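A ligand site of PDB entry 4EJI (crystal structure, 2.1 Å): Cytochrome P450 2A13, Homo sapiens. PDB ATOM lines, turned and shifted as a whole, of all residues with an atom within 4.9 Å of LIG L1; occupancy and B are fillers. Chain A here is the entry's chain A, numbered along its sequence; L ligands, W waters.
O2 of LIG L1 is in salt-bridge range of NH2 of Arg 79 (2.7 Å).
The guanidinium group (NH1) of Arg 106 lies within salt-bridge range of an oxygen (O3) of LIG L1 (2.6 Å).
O1 of LG2 L2 sits close to OD1 of Asn 275 (3.1 Å).
O3 of LIG L1 lies within salt-bridge range of NE of Arg 415, 2.8 Å away.
An oxygen (O1) of LIG L1 sits at hydrogen-bond distance from the side-chain hydroxyl of Ser 411, at 2.9 Å.
The side-chain sulfur (SG) of Cys 417 binds an iron atom (FE1) of LIG L1 (2.3 Å).
O1 of LIG L1 lies within hydrogen-bond range of NE2 of His 350, at 2.6 Å.
FE1 of LIG L1 is bound by N3 of LG2 L2 (2.1 Å).
The backbone carbonyl oxygen (O) of Ala 279 lies within hydrogen-bond range of the side-chain hydroxyl (OG1) of Thr 283.
The backbone carbonyl oxygen (O) of Arg 415 lies close to the guanidinium group (NH1) of Arg 106 (3.3 Å).
OG1 of Thr 287 is in hydrogen-bond range of O of Thr 283, 2.9 Å away.
The side-chain sulfur (SG) of Cys 417 sits close to the backbone NH (N) of Gly 419 (3.3 Å).
N of Cys 417 sits at hydrogen-bond distance from O of Phe 410, at 3.0 Å.
The guanidinium group (NH1) of Arg 415 sits at hydrogen-bond distance from the backbone carbonyl oxygen (O) of Val 94, at 3.3 Å.
The guanidinium group (NE) of Arg 79 lies within hydrogen-bond range of the backbone carbonyl oxygen (O) of Ala 95, 2.8 Å away.
The side-chain amide nitrogen (ND2) of Asn 275 sits close to the backbone NH (N) of Val 94 (3.1 Å).
Val 94 touches LIG L1.
Ala 95 touches LIG L1 (CA to O4, 3.5 Å).
CB of Ala 279 touches C23 of LIG L1 (3.5 Å).
Gly 280 touches LIG L1 (CA to C24, 3.6 Å).
Thr 283 touches LIG L1 (CB to C18, 3.4 Å).
Val 284 touches LIG L1.
Thr 287 touches LIG L1 (OG1 to C19, 3.9 Å).
NE2 of Gln 338 touches C19 of LIG L1, at 3.9 Å.
Leu 344 touches LIG L1 (CD1 to C7, 3.8 Å).
CA of Gly 347 touches C9 of LIG L1, at 3.9 Å.
Leu 348 touches LIG L1 (CB to C10, 3.8 Å).
CD1 of Leu 373 touches C9 of LIG L1, 3.5 Å away.
Pro 409 touches LIG L1 (O to C9, 3.3 Å).
Phe 410 touches LIG L1.
Phe 418 touches LIG L1 (CZ to C31, 3.3 Å).
Gly 419 touches LIG L1.
Ala 423 touches LIG L1 (CB to C18, 3.9 Å).
Hydrophobic or aromatic side chains that line LIG L1: Val 94, Ala 95, Ala 279, Val 284, Leu 344, Leu 348, His 350, Leu 373, Phe 410, Phe 418 and Ala 423.
Of the 33 residues printed, 23 come within 4 Å of LIG L1.
Water W1 bridges the side-chain hydroxyl (OG1) of Thr 287 and the side-chain amide nitrogen (NE2) of Gln 338.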
ATOM      1  N   LEU A  69     -30.598  -2.376  43.960  1.00  0.00           N
ATOM      2  CA  LEU A  69     -30.507  -2.600  42.551  1.00  0.00           C
ATOM      3  C   LEU A  69     -29.474  -3.708  42.212  1.00  0.00           C
ATOM      4  O   LEU A  69     -29.592  -4.345  41.168  1.00  0.00           O
ATOM      5  CB  LEU A  69     -30.214  -1.299  41.818  1.00  0.00           C
ATOM      6  CG  LEU A  69     -31.326  -0.507  41.096  1.00  0.00           C
ATOM      7  CD1 LEU A  69     -32.502  -0.230  41.940  1.00  0.00           C
ATOM      8  CD2 LEU A  69     -30.737   0.776  40.559  1.00  0.00           C
ATOM      9  N   ARG A  79     -39.661  -1.597  35.643  1.00  0.00           N
ATOM     10  CA  ARG A  79     -39.644  -0.192  35.163  1.00  0.00           C
ATOM     11  C   ARG A  79     -40.918   0.447  35.749  1.00  0.00           C
ATOM     12  O   ARG A  79     -42.009  -0.081  35.549  1.00  0.00           O
ATOM     13  CB  ARG A  79     -39.661  -0.130  33.639  1.00  0.00           C
ATOM     14  CG  ARG A  79     -39.845   1.278  33.016  1.00  0.00           C
ATOM     15  CD  ARG A  79     -38.623   2.186  33.325  1.00  0.00           C
ATOM     16  NE  ARG A  79     -37.406   1.676  32.719  1.00  0.00           N
ATOM     17  CZ  ARG A  79     -36.227   1.526  33.318  1.00  0.00           C
ATOM     18  NH1 ARG A  79     -35.180   1.086  32.602  1.00  0.00           N
ATOM     19  NH2 ARG A  79     -36.070   1.781  34.624  1.00  0.00           N
ATOM     20  N   VAL A  94     -37.916  -0.855  24.333  1.00  0.00           N
ATOM     21  CA  VAL A  94     -37.061  -1.456  25.340  1.00  0.00           C
ATOM     22  C   VAL A  94     -37.020  -0.772  26.730  1.00  0.00           C
ATOM     23  O   VAL A  94     -37.092  -1.459  27.778  1.00  0.00           O
ATOM     24  CB  VAL A  94     -35.643  -1.651  24.748  1.00  0.00           C
ATOM     25  CG1 VAL A  94     -35.000  -0.244  24.464  1.00  0.00           C
ATOM     26  CG2 VAL A  94     -34.838  -2.564  25.665  1.00  0.00           C
ATOM     27  N   ALA A  95     -36.884   0.568  26.727  1.00  0.00           N
ATOM     28  CA  ALA A  95     -36.681   1.398  27.923  1.00  0.00           C
ATOM     29  C   ALA A  95     -37.939   1.452  28.780  1.00  0.00           C
ATOM     30  O   ALA A  95     -37.866   1.657  29.964  1.00  0.00           O
ATOM     31  CB  ALA A  95     -36.273   2.830  27.554  1.00  0.00           C
ATOM     32  N   ARG A 106     -34.264  -6.011  25.160  1.00  0.00           N
ATOM     33  CA  ARG A 106     -32.962  -5.714  25.655  1.00  0.00           C
ATOM     34  C   ARG A 106     -31.904  -6.621  25.091  1.00  0.00           C
ATOM     35  O   ARG A 106     -30.894  -6.173  24.645  1.00  0.00           O
ATOM     36  CB  ARG A 106     -32.953  -5.790  27.183  1.00  0.00           C
ATOM     37  CG  ARG A 106     -31.604  -5.467  27.813  1.00  0.00           C
ATOM     38  CD  ARG A 106     -31.613  -5.482  29.329  1.00  0.00           C
ATOM     39  NE  ARG A 106     -30.307  -5.140  29.892  1.00  0.00           N
ATOM     40  CZ  ARG A 106     -30.049  -4.036  30.560  1.00  0.00           C
ATOM     41  NH1 ARG A 106     -31.014  -3.138  30.774  1.00  0.00           N
ATOM     42  NH2 ARG A 106     -28.829  -3.803  31.027  1.00  0.00           N
ATOM     43  N   LEU A 113     -26.757  -4.077  18.378  1.00  0.00           N
ATOM     44  CA  LEU A 113     -25.813  -2.974  18.401  1.00  0.00           C
ATOM     45  C   LEU A 113     -24.342  -3.502  18.367  1.00  0.00           C
ATOM     46  O   LEU A 113     -23.541  -2.916  17.692  1.00  0.00           O
ATOM     47  CB  LEU A 113     -26.032  -2.082  19.612  1.00  0.00           C
ATOM     48  CG  LEU A 113     -27.388  -1.355  19.685  1.00  0.00           C
ATOM     49  CD1 LEU A 113     -27.478  -0.833  21.090  1.00  0.00           C
ATOM     50  CD2 LEU A 113     -27.587  -0.216  18.642  1.00  0.00           C
ATOM     51  N   ILE A 160     -25.330   7.342  16.461  1.00  0.00           N
ATOM     52  CA  ILE A 160     -26.416   6.393  16.696  1.00  0.00           C
ATOM     53  C   ILE A 160     -27.300   6.290  15.439  1.00  0.00           C
ATOM     54  O   ILE A 160     -27.691   5.203  15.116  1.00  0.00           O
ATOM     55  CB  ILE A 160     -27.228   6.655  17.959  1.00  0.00           C
ATOM     56  CG1 ILE A 160     -28.190   5.451  18.212  1.00  0.00           C
ATOM     57  CG2 ILE A 160     -27.951   8.010  17.864  1.00  0.00           C
ATOM     58  CD1 ILE A 160     -27.547   4.085  18.567  1.00  0.00           C
ATOM     59  N   ASN A 275     -36.225   4.947  21.370  1.00  0.00           N
ATOM     60  CA  ASN A 275     -35.408   4.947  22.590  1.00  0.00           C
ATOM     61  C   ASN A 275     -33.908   5.118  22.250  1.00  0.00           C
ATOM     62  O   ASN A 275     -33.204   5.903  22.903  1.00  0.00           O
ATOM     63  CB  ASN A 275     -35.540   3.638  23.376  1.00  0.00           C
ATOM     64  CG  ASN A 275     -36.895   3.431  23.992  1.00  0.00           C
ATOM     65  OD1 ASN A 275     -37.539   4.419  24.311  1.00  0.00           O
ATOM     66  ND2 ASN A 275     -37.373   2.157  24.131  1.00  0.00           N
ATOM     67  N   LEU A 276     -33.415   4.293  21.304  1.00  0.00           N
ATOM     68  CA  LEU A 276     -32.012   4.363  20.919  1.00  0.00           C
ATOM     69  C   LEU A 276     -31.584   5.711  20.303  1.00  0.00           C
ATOM     70  O   LEU A 276     -30.542   6.225  20.646  1.00  0.00           O
ATOM     71  CB  LEU A 276     -31.588   3.208  19.998  1.00  0.00           C
ATOM     72  CG  LEU A 276     -31.958   1.803  20.434  1.00  0.00           C
ATOM     73  CD1 LEU A 276     -31.489   0.846  19.365  1.00  0.00           C
ATOM     74  CD2 LEU A 276     -31.398   1.522  21.819  1.00  0.00           C
ATOM     75  N   ALA A 279     -31.996   8.299  23.365  1.00  0.00           N
ATOM     76  CA  ALA A 279     -31.003   8.028  24.387  1.00  0.00           C
ATOM     77  C   ALA A 279     -29.577   8.234  23.833  1.00  0.00           C
ATOM     78  O   ALA A 279     -28.720   8.844  24.487  1.00  0.00           O
ATOM     79  CB  ALA A 279     -31.179   6.596  24.943  1.00  0.00           C
ATOM     80  N   GLY A 280     -29.343   7.764  22.603  1.00  0.00           N
ATOM     81  CA  GLY A 280     -28.045   7.943  21.875  1.00  0.00           C
ATOM     82  C   GLY A 280     -27.624   9.346  21.457  1.00  0.00           C
ATOM     83  O   GLY A 280     -26.472   9.559  21.039  1.00  0.00           O
ATOM     84  N   THR A 283     -27.976  12.466  25.964  1.00  0.00           N
ATOM     85  CA  THR A 283     -27.171  12.395  27.205  1.00  0.00           C
ATOM     86  C   THR A 283     -25.709  12.709  26.931  1.00  0.00           C
ATOM     87  O   THR A 283     -25.098  13.508  27.642  1.00  0.00           O
ATOM     88  CB  THR A 283     -27.305  11.033  27.964  1.00  0.00           C
ATOM     89  OG1 THR A 283     -27.589   9.971  27.037  1.00  0.00           O
ATOM     90  CG2 THR A 283     -28.422  11.084  28.991  1.00  0.00           C
ATOM     91  N   VAL A 284     -25.154  12.098  25.877  1.00  0.00           N
ATOM     92  CA  VAL A 284     -23.751  12.321  25.480  1.00  0.00           C
ATOM     93  C   VAL A 284     -23.628  13.766  25.037  1.00  0.00           C
ATOM     94  O   VAL A 284     -22.688  14.442  25.436  1.00  0.00           O
ATOM     95  CB  VAL A 284     -23.208  11.261  24.409  1.00  0.00           C
ATOM     96  CG1 VAL A 284     -21.843  11.626  23.908  1.00  0.00           C
ATOM     97  CG2 VAL A 284     -23.065   9.860  25.073  1.00  0.00           C
ATOM     98  N   THR A 287     -23.666  15.964  28.176  1.00  0.00           N
ATOM     99  CA  THR A 287     -22.434  15.715  28.934  1.00  0.00           C
ATOM    100  C   THR A 287     -21.265  16.494  28.289  1.00  0.00           C
ATOM    101  O   THR A 287     -20.501  17.200  28.975  1.00  0.00           O
ATOM    102  CB  THR A 287     -22.136  14.213  29.094  1.00  0.00           C
ATOM    103  OG1 THR A 287     -23.194  13.591  29.837  1.00  0.00           O
ATOM    104  CG2 THR A 287     -20.810  13.940  29.857  1.00  0.00           C
ATOM    105  N   GLN A 338     -18.967  13.480  34.211  1.00  0.00           N
ATOM    106  CA  GLN A 338     -20.173  12.682  34.431  1.00  0.00           C
ATOM    107  C   GLN A 338     -20.674  12.720  35.895  1.00  0.00           C
ATOM    108  O   GLN A 338     -21.829  12.763  36.086  1.00  0.00           O
ATOM    109  CB  GLN A 338     -19.927  11.269  34.021  1.00  0.00           C
ATOM    110  CG  GLN A 338     -19.580  11.170  32.547  1.00  0.00           C
ATOM    111  CD  GLN A 338     -19.776   9.741  32.056  1.00  0.00           C
ATOM    112  OE1 GLN A 338     -18.828   8.978  31.992  1.00  0.00           O
ATOM    113  NE2 GLN A 338     -21.017   9.366  31.788  1.00  0.00           N
ATOM    114  N   MET A 343     -26.380  13.787  35.016  1.00  0.00           N
ATOM    115  CA  MET A 343     -27.322  13.895  33.928  1.00  0.00           C
ATOM    116  C   MET A 343     -28.708  13.391  34.257  1.00  0.00           C
ATOM    117  O   MET A 343     -29.693  14.053  33.944  1.00  0.00           O
ATOM    118  CB  MET A 343     -26.832  13.088  32.732  1.00  0.00           C
ATOM    119  CG  MET A 343     -25.757  13.743  31.995  1.00  0.00           C
ATOM    120  SD  MET A 343     -26.410  15.258  31.290  1.00  0.00           S
ATOM    121  CE  MET A 343     -27.768  14.469  30.419  1.00  0.00           C
ATOM    122  N   LEU A 344     -28.769  12.161  34.763  1.00  0.00           N
ATOM    123  CA  LEU A 344     -30.073  11.568  35.085  1.00  0.00           C
ATOM    124  C   LEU A 344     -30.203  11.397  36.630  1.00  0.00           C
ATOM    125  O   LEU A 344     -29.920  10.315  37.133  1.00  0.00           O
ATOM    126  CB  LEU A 344     -30.201  10.243  34.351  1.00  0.00           C
ATOM    127  CG  LEU A 344     -30.392  10.246  32.830  1.00  0.00           C
ATOM    128  CD1 LEU A 344     -31.094   8.913  32.333  1.00  0.00           C
ATOM    129  CD2 LEU A 344     -31.164  11.438  32.406  1.00  0.00           C
ATOM    130  N   GLY A 347     -32.208   8.609  37.554  1.00  0.00           N
ATOM    131  CA  GLY A 347     -32.136   7.531  36.573  1.00  0.00           C
ATOM    132  C   GLY A 347     -33.472   7.490  35.885  1.00  0.00           C
ATOM    133  O   GLY A 347     -34.083   8.539  35.534  1.00  0.00           O
ATOM    134  N   LEU A 348     -33.914   6.253  35.703  1.00  0.00           N
ATOM    135  CA  LEU A 348     -35.257   5.958  35.257  1.00  0.00           C
ATOM    136  C   LEU A 348     -35.945   5.273  36.472  1.00  0.00           C
ATOM    137  O   LEU A 348     -35.289   4.578  37.263  1.00  0.00           O
ATOM    138  CB  LEU A 348     -35.189   5.061  33.997  1.00  0.00           C
ATOM    139  CG  LEU A 348     -35.423   5.472  32.534  1.00  0.00           C
ATOM    140  CD1 LEU A 348     -35.079   6.922  32.157  1.00  0.00           C
ATOM    141  CD2 LEU A 348     -34.843   4.435  31.494  1.00  0.00           C
ATOM    142  N   HIS A 350     -37.859   2.791  38.801  1.00  0.00           N
ATOM    143  CA  HIS A 350     -37.916   1.299  38.854  1.00  0.00           C
ATOM    144  C   HIS A 350     -39.239   0.852  39.502  1.00  0.00           C
ATOM    145  O   HIS A 350     -39.982   1.670  39.965  1.00  0.00           O
ATOM    146  CB  HIS A 350     -36.686   0.765  39.612  1.00  0.00           C
ATOM    147  CG  HIS A 350     -35.426   0.697  38.804  1.00  0.00           C
ATOM    148  ND1 HIS A 350     -34.728  -0.471  38.603  1.00  0.00           N
ATOM    149  CD2 HIS A 350     -34.715   1.663  38.185  1.00  0.00           C
ATOM    150  CE1 HIS A 350     -33.651  -0.217  37.872  1.00  0.00           C
ATOM    151  NE2 HIS A 350     -33.648   1.066  37.577  1.00  0.00           N
ATOM    152  N   LEU A 373     -29.723   8.251  41.918  1.00  0.00           N
ATOM    153  CA  LEU A 373     -28.386   8.134  41.395  1.00  0.00           C
ATOM    154  C   LEU A 373     -27.583   9.393  41.711  1.00  0.00           C
ATOM    155  O   LEU A 373     -26.409   9.283  42.083  1.00  0.00           O
ATOM    156  CB  LEU A 373     -28.433   7.889  39.883  1.00  0.00           C
ATOM    157  CG  LEU A 373     -29.189   6.654  39.339  1.00  0.00           C
ATOM    158  CD1 LEU A 373     -28.909   6.529  37.811  1.00  0.00           C
ATOM    159  CD2 LEU A 373     -28.787   5.435  40.023  1.00  0.00           C
ATOM    160  N   PRO A 409     -23.418   6.805  36.974  1.00  0.00           N
ATOM    161  CA  PRO A 409     -24.330   7.616  36.136  1.00  0.00           C
ATOM    162  C   PRO A 409     -25.124   6.827  35.081  1.00  0.00           C
ATOM    163  O   PRO A 409     -26.101   7.358  34.564  1.00  0.00           O
ATOM    164  CB  PRO A 409     -23.413   8.624  35.446  1.00  0.00           C
ATOM    165  CG  PRO A 409     -22.119   7.828  35.273  1.00  0.00           C
ATOM    166  CD  PRO A 409     -22.005   6.958  36.518  1.00  0.00           C
ATOM    167  N   PHE A 410     -24.672   5.615  34.795  1.00  0.00           N
ATOM    168  CA  PHE A 410     -25.394   4.665  33.956  1.00  0.00           C
ATOM    169  C   PHE A 410     -26.279   3.722  34.745  1.00  0.00           C
ATOM    170  O   PHE A 410     -26.769   2.766  34.215  1.00  0.00           O
ATOM    171  CB  PHE A 410     -24.384   3.815  33.143  1.00  0.00           C
ATOM    172  CG  PHE A 410     -23.504   4.646  32.261  1.00  0.00           C
ATOM    173  CD1 PHE A 410     -24.007   5.175  31.046  1.00  0.00           C
ATOM    174  CD2 PHE A 410     -22.180   4.930  32.658  1.00  0.00           C
ATOM    175  CE1 PHE A 410     -23.186   5.997  30.232  1.00  0.00           C
ATOM    176  CE2 PHE A 410     -21.325   5.716  31.834  1.00  0.00           C
ATOM    177  CZ  PHE A 410     -21.832   6.280  30.660  1.00  0.00           C
ATOM    178  N   SER A 411     -26.458   4.000  36.030  1.00  0.00           N
ATOM    179  CA  SER A 411     -27.196   3.088  36.950  1.00  0.00           C
ATOM    180  C   SER A 411     -26.476   1.750  37.099  1.00  0.00           C
ATOM    181  O   SER A 411     -25.329   1.623  36.719  1.00  0.00           O
ATOM    182  CB  SER A 411     -28.687   2.922  36.569  1.00  0.00           C
ATOM    183  OG  SER A 411     -29.399   2.353  37.665  1.00  0.00           O
ATOM    184  N   ILE A 412     -27.137   0.790  37.718  1.00  0.00           N
ATOM    185  CA  ILE A 412     -26.504  -0.500  38.078  1.00  0.00           C
ATOM    186  C   ILE A 412     -27.631  -1.515  38.147  1.00  0.00           C
ATOM    187  O   ILE A 412     -28.772  -1.119  38.147  1.00  0.00           O
ATOM    188  CB  ILE A 412     -25.820  -0.489  39.437  1.00  0.00           C
ATOM    189  CG1 ILE A 412     -26.762   0.149  40.452  1.00  0.00           C
ATOM    190  CG2 ILE A 412     -24.426   0.263  39.372  1.00  0.00           C
ATOM    191  CD1 ILE A 412     -26.208   0.150  41.905  1.00  0.00           C
ATOM    192  N   ARG A 415     -31.184  -3.475  34.933  1.00  0.00           N
ATOM    193  CA  ARG A 415     -31.664  -2.505  33.945  1.00  0.00           C
ATOM    194  C   ARG A 415     -30.608  -1.480  33.559  1.00  0.00           C
ATOM    195  O   ARG A 415     -30.932  -0.544  32.847  1.00  0.00           O
ATOM    196  CB  ARG A 415     -32.934  -1.747  34.412  1.00  0.00           C
ATOM    197  CG  ARG A 415     -34.206  -2.581  34.619  1.00  0.00           C
ATOM    198  CD  ARG A 415     -34.660  -3.494  33.453  1.00  0.00           C
ATOM    199  NE  ARG A 415     -35.242  -2.743  32.336  1.00  0.00           N
ATOM    200  CZ  ARG A 415     -36.555  -2.578  32.127  1.00  0.00           C
ATOM    201  NH1 ARG A 415     -36.995  -1.908  31.093  1.00  0.00           N
ATOM    202  NH2 ARG A 415     -37.445  -3.098  32.978  1.00  0.00           N
ATOM    203  N   TYR A 416     -29.363  -1.672  33.996  1.00  0.00           N
ATOM    204  CA  TYR A 416     -28.301  -0.693  33.744  1.00  0.00           C
ATOM    205  C   TYR A 416     -28.255  -0.268  32.257  1.00  0.00           C
ATOM    206  O   TYR A 416     -28.597  -1.040  31.349  1.00  0.00           O
ATOM    207  CB  TYR A 416     -26.921  -1.145  34.319  1.00  0.00           C
ATOM    208  CG  TYR A 416     -26.139  -1.950  33.364  1.00  0.00           C
ATOM    209  CD1 TYR A 416     -25.231  -1.333  32.528  1.00  0.00           C
ATOM    210  CD2 TYR A 416     -26.369  -3.344  33.210  1.00  0.00           C
ATOM    211  CE1 TYR A 416     -24.508  -2.068  31.556  1.00  0.00           C
ATOM    212  CE2 TYR A 416     -25.677  -4.079  32.251  1.00  0.00           C
ATOM    213  CZ  TYR A 416     -24.747  -3.401  31.434  1.00  0.00           C
ATOM    214  OH  TYR A 416     -24.041  -4.013  30.483  1.00  0.00           O
ATOM    215  N   CYS A 417     -27.811   0.959  32.028  1.00  0.00           N
ATOM    216  CA  CYS A 417     -27.731   1.513  30.674  1.00  0.00           C
ATOM    217  C   CYS A 417     -26.830   0.642  29.744  1.00  0.00           C
ATOM    218  O   CYS A 417     -25.637   0.620  29.911  1.00  0.00           O
ATOM    219  CB  CYS A 417     -27.236   2.962  30.703  1.00  0.00           C
ATOM    220  SG  CYS A 417     -26.970   3.631  29.069  1.00  0.00           S
ATOM    221  N   PHE A 418     -27.450  -0.081  28.824  1.00  0.00           N
ATOM    222  CA  PHE A 418     -26.657  -0.894  27.909  1.00  0.00           C
ATOM    223  C   PHE A 418     -26.019   0.017  26.815  1.00  0.00           C
ATOM    224  O   PHE A 418     -25.271  -0.457  26.045  1.00  0.00           O
ATOM    225  CB  PHE A 418     -27.398  -2.159  27.337  1.00  0.00           C
ATOM    226  CG  PHE A 418     -28.598  -1.849  26.428  1.00  0.00           C
ATOM    227  CD1 PHE A 418     -28.406  -1.461  25.093  1.00  0.00           C
ATOM    228  CD2 PHE A 418     -29.921  -1.990  26.906  1.00  0.00           C
ATOM    229  CE1 PHE A 418     -29.468  -1.206  24.236  1.00  0.00           C
ATOM    230  CE2 PHE A 418     -31.004  -1.734  26.063  1.00  0.00           C
ATOM    231  CZ  PHE A 418     -30.809  -1.363  24.718  1.00  0.00           C
ATOM    232  N   GLY A 419     -26.251   1.321  26.830  1.00  0.00           N
ATOM    233  CA  GLY A 419     -25.480   2.209  25.986  1.00  0.00           C
ATOM    234  C   GLY A 419     -24.162   2.620  26.595  1.00  0.00           C
ATOM    235  O   GLY A 419     -23.417   3.396  25.999  1.00  0.00           O
ATOM    236  N   LEU A 422     -20.859   2.283  24.539  1.00  0.00           N
ATOM    237  CA  LEU A 422     -20.889   3.282  23.501  1.00  0.00           C
ATOM    238  C   LEU A 422     -20.685   4.725  24.010  1.00  0.00           C
ATOM    239  O   LEU A 422     -19.946   5.473  23.401  1.00  0.00           O
ATOM    240  CB  LEU A 422     -22.205   3.245  22.725  1.00  0.00           C
ATOM    241  CG  LEU A 422     -22.284   4.314  21.648  1.00  0.00           C
ATOM    242  CD1 LEU A 422     -21.195   4.251  20.572  1.00  0.00           C
ATOM    243  CD2 LEU A 422     -23.646   4.168  21.066  1.00  0.00           C
ATOM    244  N   ALA A 423     -21.412   5.106  25.069  1.00  0.00           N
ATOM    245  CA  ALA A 423     -21.231   6.414  25.678  1.00  0.00           C
ATOM    246  C   ALA A 423     -19.742   6.669  26.083  1.00  0.00           C
ATOM    247  O   ALA A 423     -19.215   7.732  25.752  1.00  0.00           O
ATOM    248  CB  ALA A 423     -22.123   6.595  26.882  1.00  0.00           C
ATOM    249  N   LEU A 427     -17.496   9.625  24.665  1.00  0.00           N
ATOM    250  CA  LEU A 427     -17.001  10.688  25.556  1.00  0.00           C
ATOM    251  C   LEU A 427     -15.482  10.795  25.430  1.00  0.00           C
ATOM    252  O   LEU A 427     -14.948  11.880  25.212  1.00  0.00           O
ATOM    253  CB  LEU A 427     -17.418  10.477  26.998  1.00  0.00           C
ATOM    254  CG  LEU A 427     -18.942  10.712  27.121  1.00  0.00           C
ATOM    255  CD1 LEU A 427     -19.449  10.192  28.499  1.00  0.00           C
ATOM    256  CD2 LEU A 427     -19.273  12.160  26.991  1.00  0.00           C
HETATM  257  C1  LIG L   1     -31.116   3.480  30.545  1.00  0.00           C
HETATM  258  C2  LIG L   1     -27.749   6.711  31.733  1.00  0.00           C
HETATM  259  C3  LIG L   1     -26.213   6.794  27.103  1.00  0.00           C
HETATM  260  C4  LIG L   1     -29.652   3.567  25.888  1.00  0.00           C
HETATM  261  C5  LIG L   1     -30.367   4.377  31.275  1.00  0.00           C
HETATM  262  C6  LIG L   1     -30.479   4.607  32.711  1.00  0.00           C
HETATM  263  C7  LIG L   1     -29.526   5.488  33.047  1.00  0.00           C
HETATM  264  C8  LIG L   1     -28.792   5.819  31.826  1.00  0.00           C
HETATM  265  C9  LIG L   1     -29.198   6.134  34.387  1.00  0.00           C
HETATM  266  C10 LIG L   1     -31.549   3.918  33.599  1.00  0.00           C
HETATM  267  C11 LIG L   1     -31.205   2.452  33.832  1.00  0.00           C
HETATM  268  C12 LIG L   1     -32.181   1.966  34.876  1.00  0.00           C
HETATM  269  O1  LIG L   1     -31.785   1.943  36.056  1.00  0.00           O
HETATM  270  O2  LIG L   1     -33.354   1.687  34.551  1.00  0.00           O
HETATM  271  C13 LIG L   1     -27.064   7.106  30.594  1.00  0.00           C
HETATM  272  C14 LIG L   1     -26.042   8.157  30.495  1.00  0.00           C
HETATM  273  C15 LIG L   1     -25.656   8.146  29.188  1.00  0.00           C
HETATM  274  C16 LIG L   1     -26.345   7.094  28.464  1.00  0.00           C
HETATM  275  C17 LIG L   1     -25.614   9.122  31.643  1.00  0.00           C
HETATM  276  C18 LIG L   1     -24.654   9.044  28.469  1.00  0.00           C
HETATM  277  C19 LIG L   1     -23.789   9.827  29.099  1.00  0.00           C
HETATM  278  C20 LIG L   1     -26.998   5.937  26.373  1.00  0.00           C
HETATM  279  C21 LIG L   1     -26.872   5.600  24.971  1.00  0.00           C
HETATM  280  C22 LIG L   1     -27.817   4.733  24.631  1.00  0.00           C
HETATM  281  C23 LIG L   1     -28.575   4.427  25.821  1.00  0.00           C
HETATM  282  C24 LIG L   1     -25.826   6.165  24.031  1.00  0.00           C
HETATM  283  C25 LIG L   1     -28.050   4.133  23.229  1.00  0.00           C
HETATM  284  C26 LIG L   1     -27.606   2.905  23.014  1.00  0.00           C
HETATM  285  C27 LIG L   1     -30.344   3.226  27.010  1.00  0.00           C
HETATM  286  C28 LIG L   1     -31.475   2.310  27.018  1.00  0.00           C
HETATM  287  C29 LIG L   1     -31.933   2.264  28.458  1.00  0.00           C
HETATM  288  C30 LIG L   1     -31.055   3.178  29.188  1.00  0.00           C
HETATM  289  C31 LIG L   1     -32.069   1.546  25.793  1.00  0.00           C
HETATM  290  C32 LIG L   1     -33.062   1.407  29.003  1.00  0.00           C
HETATM  291  C33 LIG L   1     -32.490   0.045  29.421  1.00  0.00           C
HETATM  292  C34 LIG L   1     -33.577  -0.823  30.060  1.00  0.00           C
HETATM  293  O3  LIG L   1     -33.321  -2.005  30.423  1.00  0.00           O
HETATM  294  O4  LIG L   1     -34.730  -0.332  30.245  1.00  0.00           O
HETATM  295  N1  LIG L   1     -29.324   5.118  30.777  1.00  0.00           N
HETATM  296  N2  LIG L   1     -27.198   6.520  29.340  1.00  0.00           N
HETATM  297  N3  LIG L   1     -28.051   5.199  26.840  1.00  0.00           N
HETATM  298  N4  LIG L   1     -30.158   3.719  28.302  1.00  0.00           N
HETATM  299 FE1  LIG L   1     -28.704   5.163  28.818  1.00  0.00          FE
HETATM  300  O1  LG2 L   2     -37.257   7.495  23.923  1.00  0.00           O
HETATM  301  N1  LG2 L   2     -36.860   7.616  25.065  1.00  0.00           N
HETATM  302  N2  LG2 L   2     -36.978   8.817  25.650  1.00  0.00           N
HETATM  303  C1  LG2 L   2     -38.040   9.694  25.104  1.00  0.00           C
HETATM  304  C2  LG2 L   2     -37.232   8.595  27.087  1.00  0.00           C
HETATM  305  C3  LG2 L   2     -36.174   7.756  27.799  1.00  0.00           C
HETATM  306  C4  LG2 L   2     -34.770   7.744  27.179  1.00  0.00           C
HETATM  307  C5  LG2 L   2     -33.834   6.988  28.112  1.00  0.00           C
HETATM  308  O2  LG2 L   2     -34.192   6.023  28.753  1.00  0.00           O
HETATM  309  C6  LG2 L   2     -32.420   7.356  28.242  1.00  0.00           C
HETATM  310  C7  LG2 L   2     -32.018   8.674  28.153  1.00  0.00           C
HETATM  311  C8  LG2 L   2     -30.632   8.867  28.261  1.00  0.00           C
HETATM  312  C9  LG2 L   2     -29.774   7.790  28.446  1.00  0.00           C
HETATM  313  N3  LG2 L   2     -30.195   6.535  28.478  1.00  0.00           N
HETATM  314  C10 LG2 L   2     -31.500   6.338  28.396  1.00  0.00           C
HETATM  315  O   HOH W   1     -22.866  11.614  31.791  1.00  0.00           O
